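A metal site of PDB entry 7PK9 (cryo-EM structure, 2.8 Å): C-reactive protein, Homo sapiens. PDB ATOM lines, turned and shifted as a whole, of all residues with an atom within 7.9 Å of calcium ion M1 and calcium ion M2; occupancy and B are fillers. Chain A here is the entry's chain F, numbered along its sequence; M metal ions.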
ATOM      1  N   SER A  50     -11.474  -0.081   3.964  1.00  0.00           N
ATOM      2  CA  SER A  50     -12.848  -0.200   4.415  1.00  0.00           C
ATOM      3  C   SER A  50     -13.026   0.170   5.884  1.00  0.00           C
ATOM      4  O   SER A  50     -12.386  -0.421   6.758  1.00  0.00           O
ATOM      5  CB  SER A  50     -13.344  -1.623   4.199  1.00  0.00           C
ATOM      6  OG  SER A  50     -14.642  -1.783   4.727  1.00  0.00           O
ATOM      7  N   SER A  53     -18.290  -2.240   6.315  1.00  0.00           N
ATOM      8  CA  SER A  53     -18.695  -3.036   5.164  1.00  0.00           C
ATOM      9  C   SER A  53     -19.874  -3.920   5.565  1.00  0.00           C
ATOM     10  O   SER A  53     -19.714  -4.862   6.349  1.00  0.00           O
ATOM     11  CB  SER A  53     -17.521  -3.863   4.646  1.00  0.00           C
ATOM     12  OG  SER A  53     -17.936  -4.767   3.645  1.00  0.00           O
ATOM     13  N   TYR A  54     -21.051  -3.600   5.034  1.00  0.00           N
ATOM     14  CA  TYR A  54     -22.296  -4.332   5.249  1.00  0.00           C
ATOM     15  C   TYR A  54     -22.722  -4.991   3.945  1.00  0.00           C
ATOM     16  O   TYR A  54     -22.920  -4.302   2.940  1.00  0.00           O
ATOM     17  CB  TYR A  54     -23.347  -3.327   5.735  1.00  0.00           C
ATOM     18  CG  TYR A  54     -24.748  -3.808   6.000  1.00  0.00           C
ATOM     19  CD1 TYR A  54     -25.566  -4.240   4.975  1.00  0.00           C
ATOM     20  CD2 TYR A  54     -25.286  -3.741   7.270  1.00  0.00           C
ATOM     21  CE1 TYR A  54     -26.848  -4.629   5.208  1.00  0.00           C
ATOM     22  CE2 TYR A  54     -26.576  -4.136   7.512  1.00  0.00           C
ATOM     23  CZ  TYR A  54     -27.354  -4.577   6.471  1.00  0.00           C
ATOM     24  OH  TYR A  54     -28.645  -4.992   6.692  1.00  0.00           O
ATOM     25  N   ALA A  55     -22.876  -6.306   3.957  1.00  0.00           N
ATOM     26  CA  ALA A  55     -23.235  -7.065   2.765  1.00  0.00           C
ATOM     27  C   ALA A  55     -24.463  -7.919   2.982  1.00  0.00           C
ATOM     28  O   ALA A  55     -24.650  -8.500   4.046  1.00  0.00           O
ATOM     29  CB  ALA A  55     -22.090  -7.975   2.331  1.00  0.00           C
ATOM     30  N   GLN A  59     -25.868  -8.590  -2.643  1.00  0.00           N
ATOM     31  CA  GLN A  59     -25.200  -7.317  -2.873  1.00  0.00           C
ATOM     32  C   GLN A  59     -24.072  -7.190  -1.863  1.00  0.00           C
ATOM     33  O   GLN A  59     -24.341  -7.049  -0.666  1.00  0.00           O
ATOM     34  CB  GLN A  59     -26.192  -6.180  -2.742  1.00  0.00           C
ATOM     35  CG  GLN A  59     -25.630  -4.811  -2.947  1.00  0.00           C
ATOM     36  CD  GLN A  59     -24.922  -4.680  -4.262  1.00  0.00           C
ATOM     37  OE1 GLN A  59     -23.695  -4.775  -4.337  1.00  0.00           O
ATOM     38  NE2 GLN A  59     -25.696  -4.469  -5.322  1.00  0.00           N
ATOM     39  N   ASP A  60     -22.825  -7.283  -2.305  1.00  0.00           N
ATOM     40  CA  ASP A  60     -21.696  -7.258  -1.379  1.00  0.00           C
ATOM     41  C   ASP A  60     -21.394  -5.864  -0.850  1.00  0.00           C
ATOM     42  O   ASP A  60     -20.780  -5.744   0.210  1.00  0.00           O
ATOM     43  CB  ASP A  60     -20.452  -7.848  -2.027  1.00  0.00           C
ATOM     44  CG  ASP A  60     -19.932  -6.994  -3.187  1.00  0.00           C
ATOM     45  OD1 ASP A  60     -18.785  -6.523  -3.119  1.00  0.00           O
ATOM     46  OD2 ASP A  60     -20.678  -6.805  -4.171  1.00  0.00           O
ATOM     47  N   ASN A  61     -21.809  -4.811  -1.549  1.00  0.00           N
ATOM     48  CA  ASN A  61     -21.564  -3.446  -1.108  1.00  0.00           C
ATOM     49  C   ASN A  61     -22.891  -2.833  -0.711  1.00  0.00           C
ATOM     50  O   ASN A  61     -23.265  -1.778  -1.232  1.00  0.00           O
ATOM     51  CB  ASN A  61     -20.909  -2.616  -2.205  1.00  0.00           C
ATOM     52  CG  ASN A  61     -19.628  -3.216  -2.687  1.00  0.00           C
ATOM     53  OD1 ASN A  61     -18.975  -3.969  -1.977  1.00  0.00           O
ATOM     54  ND2 ASN A  61     -19.260  -2.896  -3.917  1.00  0.00           N
ATOM     55  N   GLU A  62     -23.618  -3.486   0.173  1.00  0.00           N
ATOM     56  CA  GLU A  62     -24.981  -3.048   0.441  1.00  0.00           C
ATOM     57  C   GLU A  62     -25.014  -1.763   1.249  1.00  0.00           C
ATOM     58  O   GLU A  62     -25.801  -0.866   0.949  1.00  0.00           O
ATOM     59  CB  GLU A  62     -25.733  -4.161   1.158  1.00  0.00           C
ATOM     60  CG  GLU A  62     -27.167  -3.834   1.460  1.00  0.00           C
ATOM     61  CD  GLU A  62     -27.994  -3.832   0.207  1.00  0.00           C
ATOM     62  OE1 GLU A  62     -27.487  -4.287  -0.835  1.00  0.00           O
ATOM     63  OE2 GLU A  62     -29.158  -3.406   0.256  1.00  0.00           O
ATOM     64  N   LEU A  64     -21.495   0.487   2.342  1.00  0.00           N
ATOM     65  CA  LEU A  64     -20.060   0.527   2.534  1.00  0.00           C
ATOM     66  C   LEU A  64     -19.609   1.950   2.785  1.00  0.00           C
ATOM     67  O   LEU A  64     -19.963   2.863   2.020  1.00  0.00           O
ATOM     68  CB  LEU A  64     -19.339  -0.072   1.327  1.00  0.00           C
ATOM     69  CG  LEU A  64     -17.821  -0.045   1.304  1.00  0.00           C
ATOM     70  CD1 LEU A  64     -17.225  -1.031   2.285  1.00  0.00           C
ATOM     71  CD2 LEU A  64     -17.337  -0.334  -0.099  1.00  0.00           C
ATOM     72  N   PHE A  66     -16.135   3.740   2.881  1.00  0.00           N
ATOM     73  CA  PHE A  66     -14.809   3.424   2.370  1.00  0.00           C
ATOM     74  C   PHE A  66     -14.006   4.715   2.228  1.00  0.00           C
ATOM     75  O   PHE A  66     -14.475   5.670   1.614  1.00  0.00           O
ATOM     76  CB  PHE A  66     -14.931   2.711   1.024  1.00  0.00           C
ATOM     77  CG  PHE A  66     -13.707   1.979   0.603  1.00  0.00           C
ATOM     78  CD1 PHE A  66     -13.549   0.654   0.912  1.00  0.00           C
ATOM     79  CD2 PHE A  66     -12.743   2.600  -0.161  1.00  0.00           C
ATOM     80  CE1 PHE A  66     -12.429  -0.025   0.500  1.00  0.00           C
ATOM     81  CE2 PHE A  66     -11.636   1.923  -0.561  1.00  0.00           C
ATOM     82  CZ  PHE A  66     -11.477   0.617  -0.230  1.00  0.00           C
ATOM     83  N   THR A  76     -21.392   4.235  -0.244  1.00  0.00           N
ATOM     84  CA  THR A  76     -22.223   3.544  -1.210  1.00  0.00           C
ATOM     85  C   THR A  76     -23.261   2.699  -0.506  1.00  0.00           C
ATOM     86  O   THR A  76     -23.008   2.074   0.531  1.00  0.00           O
ATOM     87  CB  THR A  76     -21.404   2.638  -2.133  1.00  0.00           C
ATOM     88  OG1 THR A  76     -22.283   1.935  -3.013  1.00  0.00           O
ATOM     89  CG2 THR A  76     -20.617   1.635  -1.369  1.00  0.00           C
ATOM     90  N   GLN A 137     -12.502  -5.256   7.166  1.00  0.00           N
ATOM     91  CA  GLN A 137     -12.308  -5.774   5.828  1.00  0.00           C
ATOM     92  C   GLN A 137     -13.395  -5.205   4.933  1.00  0.00           C
ATOM     93  O   GLN A 137     -14.466  -4.828   5.391  1.00  0.00           O
ATOM     94  CB  GLN A 137     -12.388  -7.306   5.783  1.00  0.00           C
ATOM     95  CG  GLN A 137     -11.405  -8.029   6.651  1.00  0.00           C
ATOM     96  CD  GLN A 137      -9.981  -7.879   6.198  1.00  0.00           C
ATOM     97  OE1 GLN A 137      -9.719  -7.555   5.042  1.00  0.00           O
ATOM     98  NE2 GLN A 137      -9.044  -8.133   7.091  1.00  0.00           N
ATOM     99  N   GLU A 138     -13.116  -5.200   3.632  1.00  0.00           N
ATOM    100  CA  GLU A 138     -14.133  -4.995   2.621  1.00  0.00           C
ATOM    101  C   GLU A 138     -14.470  -6.354   2.049  1.00  0.00           C
ATOM    102  O   GLU A 138     -13.587  -7.056   1.551  1.00  0.00           O
ATOM    103  CB  GLU A 138     -13.639  -4.060   1.515  1.00  0.00           C
ATOM    104  CG  GLU A 138     -14.723  -3.257   0.832  1.00  0.00           C
ATOM    105  CD  GLU A 138     -15.560  -4.087  -0.120  1.00  0.00           C
ATOM    106  OE1 GLU A 138     -14.986  -4.717  -1.030  1.00  0.00           O
ATOM    107  OE2 GLU A 138     -16.795  -4.106   0.023  1.00  0.00           O
ATOM    108  N   GLN A 139     -15.732  -6.731   2.109  1.00  0.00           N
ATOM    109  CA  GLN A 139     -16.150  -8.047   1.664  1.00  0.00           C
ATOM    110  C   GLN A 139     -16.729  -7.980   0.259  1.00  0.00           C
ATOM    111  O   GLN A 139     -17.536  -7.107  -0.042  1.00  0.00           O
ATOM    112  CB  GLN A 139     -17.116  -8.670   2.672  1.00  0.00           C
ATOM    113  CG  GLN A 139     -18.508  -8.145   2.710  1.00  0.00           C
ATOM    114  CD  GLN A 139     -19.100  -8.324   4.087  1.00  0.00           C
ATOM    115  OE1 GLN A 139     -19.040  -9.403   4.652  1.00  0.00           O
ATOM    116  NE2 GLN A 139     -19.692  -7.273   4.636  1.00  0.00           N
ATOM    117  N   ASP A 140     -16.300  -8.918  -0.582  1.00  0.00           N
ATOM    118  CA  ASP A 140     -16.767  -9.028  -1.952  1.00  0.00           C
ATOM    119  C   ASP A 140     -17.700 -10.208  -2.166  1.00  0.00           C
ATOM    120  O   ASP A 140     -18.292 -10.324  -3.238  1.00  0.00           O
ATOM    121  CB  ASP A 140     -15.575  -9.158  -2.911  1.00  0.00           C
ATOM    122  CG  ASP A 140     -14.811  -7.862  -3.078  1.00  0.00           C
ATOM    123  OD1 ASP A 140     -13.588  -7.903  -3.257  1.00  0.00           O
ATOM    124  OD2 ASP A 140     -15.453  -6.800  -3.039  1.00  0.00           O
ATOM    125  N   SER A 141     -17.860 -11.059  -1.161  1.00  0.00           N
ATOM    126  CA  SER A 141     -18.929 -12.045  -1.101  1.00  0.00           C
ATOM    127  C   SER A 141     -19.548 -11.955   0.283  1.00  0.00           C
ATOM    128  O   SER A 141     -19.033 -11.275   1.162  1.00  0.00           O
ATOM    129  CB  SER A 141     -18.425 -13.466  -1.383  1.00  0.00           C
ATOM    130  OG  SER A 141     -17.537 -13.917  -0.378  1.00  0.00           O
ATOM    131  N   GLY A 144     -16.821 -12.982   2.937  1.00  0.00           N
ATOM    132  CA  GLY A 144     -15.454 -13.351   2.637  1.00  0.00           C
ATOM    133  C   GLY A 144     -14.934 -12.671   1.395  1.00  0.00           C
ATOM    134  O   GLY A 144     -15.441 -11.625   0.980  1.00  0.00           O
ATOM    135  N   ASN A 145     -13.903 -13.275   0.810  1.00  0.00           N
ATOM    136  CA  ASN A 145     -13.139 -12.656  -0.266  1.00  0.00           C
ATOM    137  C   ASN A 145     -12.597 -11.293   0.150  1.00  0.00           C
ATOM    138  O   ASN A 145     -12.793 -10.287  -0.530  1.00  0.00           O
ATOM    139  CB  ASN A 145     -13.965 -12.564  -1.548  1.00  0.00           C
ATOM    140  CG  ASN A 145     -14.239 -13.913  -2.156  1.00  0.00           C
ATOM    141  OD1 ASN A 145     -15.218 -14.574  -1.831  1.00  0.00           O
ATOM    142  ND2 ASN A 145     -13.352 -14.342  -3.046  1.00  0.00           N
ATOM    143  N   PHE A 146     -11.939 -11.258   1.295  1.00  0.00           N
ATOM    144  CA  PHE A 146     -11.298 -10.049   1.771  1.00  0.00           C
ATOM    145  C   PHE A 146      -9.984  -9.814   1.037  1.00  0.00           C
ATOM    146  O   PHE A 146      -9.291 -10.752   0.653  1.00  0.00           O
ATOM    147  CB  PHE A 146     -11.043 -10.122   3.274  1.00  0.00           C
ATOM    148  CG  PHE A 146     -12.229 -10.539   4.061  1.00  0.00           C
ATOM    149  CD1 PHE A 146     -13.431  -9.873   3.932  1.00  0.00           C
ATOM    150  CD2 PHE A 146     -12.152 -11.588   4.942  1.00  0.00           C
ATOM    151  CE1 PHE A 146     -14.514 -10.250   4.660  1.00  0.00           C
ATOM    152  CE2 PHE A 146     -13.249 -11.961   5.673  1.00  0.00           C
ATOM    153  CZ  PHE A 146     -14.425 -11.301   5.530  1.00  0.00           C
ATOM    154  N   GLU A 147      -9.646  -8.539   0.847  1.00  0.00           N
ATOM    155  CA  GLU A 147      -8.401  -8.151   0.202  1.00  0.00           C
ATOM    156  C   GLU A 147      -7.556  -7.387   1.206  1.00  0.00           C
ATOM    157  O   GLU A 147      -7.980  -6.361   1.742  1.00  0.00           O
ATOM    158  CB  GLU A 147      -8.681  -7.269  -1.012  1.00  0.00           C
ATOM    159  CG  GLU A 147      -9.463  -7.968  -2.086  1.00  0.00           C
ATOM    160  CD  GLU A 147      -9.890  -7.032  -3.184  1.00  0.00           C
ATOM    161  OE1 GLU A 147      -9.643  -5.820  -3.048  1.00  0.00           O
ATOM    162  OE2 GLU A 147     -10.483  -7.500  -4.169  1.00  0.00           O
ATOM    163  N   SER A 149      -5.080  -5.487   0.763  1.00  0.00           N
ATOM    164  CA  SER A 149      -4.894  -4.114   0.328  1.00  0.00           C
ATOM    165  C   SER A 149      -6.073  -3.215   0.653  1.00  0.00           C
ATOM    166  O   SER A 149      -5.978  -2.006   0.452  1.00  0.00           O
ATOM    167  CB  SER A 149      -4.625  -4.087  -1.172  1.00  0.00           C
ATOM    168  OG  SER A 149      -5.726  -4.613  -1.891  1.00  0.00           O
ATOM    169  N   GLN A 150      -7.183  -3.771   1.118  1.00  0.00           N
ATOM    170  CA  GLN A 150      -8.326  -2.996   1.575  1.00  0.00           C
ATOM    171  C   GLN A 150      -8.609  -3.137   3.062  1.00  0.00           C
ATOM    172  O   GLN A 150      -9.568  -2.540   3.546  1.00  0.00           O
ATOM    173  CB  GLN A 150      -9.577  -3.385   0.779  1.00  0.00           C
ATOM    174  CG  GLN A 150      -9.508  -3.035  -0.686  1.00  0.00           C
ATOM    175  CD  GLN A 150     -10.838  -3.176  -1.360  1.00  0.00           C
ATOM    176  OE1 GLN A 150     -11.582  -4.101  -1.076  1.00  0.00           O
ATOM    177  NE2 GLN A 150     -11.156  -2.232  -2.227  1.00  0.00           N
HETATM  178 CA    CA M   1     -13.126  -5.753  -2.193  1.00  0.00          CA
HETATM  179 CA    CA M   2     -16.960  -5.171  -2.074  1.00  0.00          CA
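Calcium ion M2 is bound by the side-chain carboxylate (OE1) of Glu 138 (2.3 Å), the side-chain amide oxygen (OD1) of Asn 61 (2.3 Å), the side-chain carboxylate (OE2) of Glu 138 (2.4 Å), the side-chain carboxylate (OD2) of Asp 140 (2.4 Å), the side-chain carboxylate (OD1) of Asp 60 (2.5 Å) and the backbone carbonyl oxygen (O) of Gln 139 (2.9 Å). Calcium ion M2 has six donor atoms within binding distance.
The backbone NH (N) of Ala 55 sits close to the side-chain amide nitrogen (NE2) of Gln 139 (3.4 Å). The backbone NH (N) of Asn 61 sits close to the side-chain amide oxygen (OE1) of Gln 59 (3.4 Å). The side-chain amide nitrogen of Gln 139 sits at hydrogen-bond distance from the backbone carbonyl oxygen of Ser 53, at 3.0 Å. The side-chain carboxylate (OE1) of Glu 147 sits close to the side-chain amide oxygen (OE1) of Gln 150 (3.3 Å). N of Ser 50 lies within hydrogen-bond range of O of Gln 150, 3.1 Å away.
Five residues have an atom within 4 Å of calcium ion M2: Asp 60, Asn 61, Glu 138, Gln 139 and Asp 140.
Calcium ion M1 is bound by OE1 of Glu 138, OD1 of Asp 140, OE1 of Gln 150 and OD2 of Asp 140. Calcium ion M1 has four donor atoms within binding distance.
Glu 147 touches calcium ion M1. Four residues have an atom within 4 Å of calcium ion M1: Glu 138, Asp 140, Glu 147 and Gln 150.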
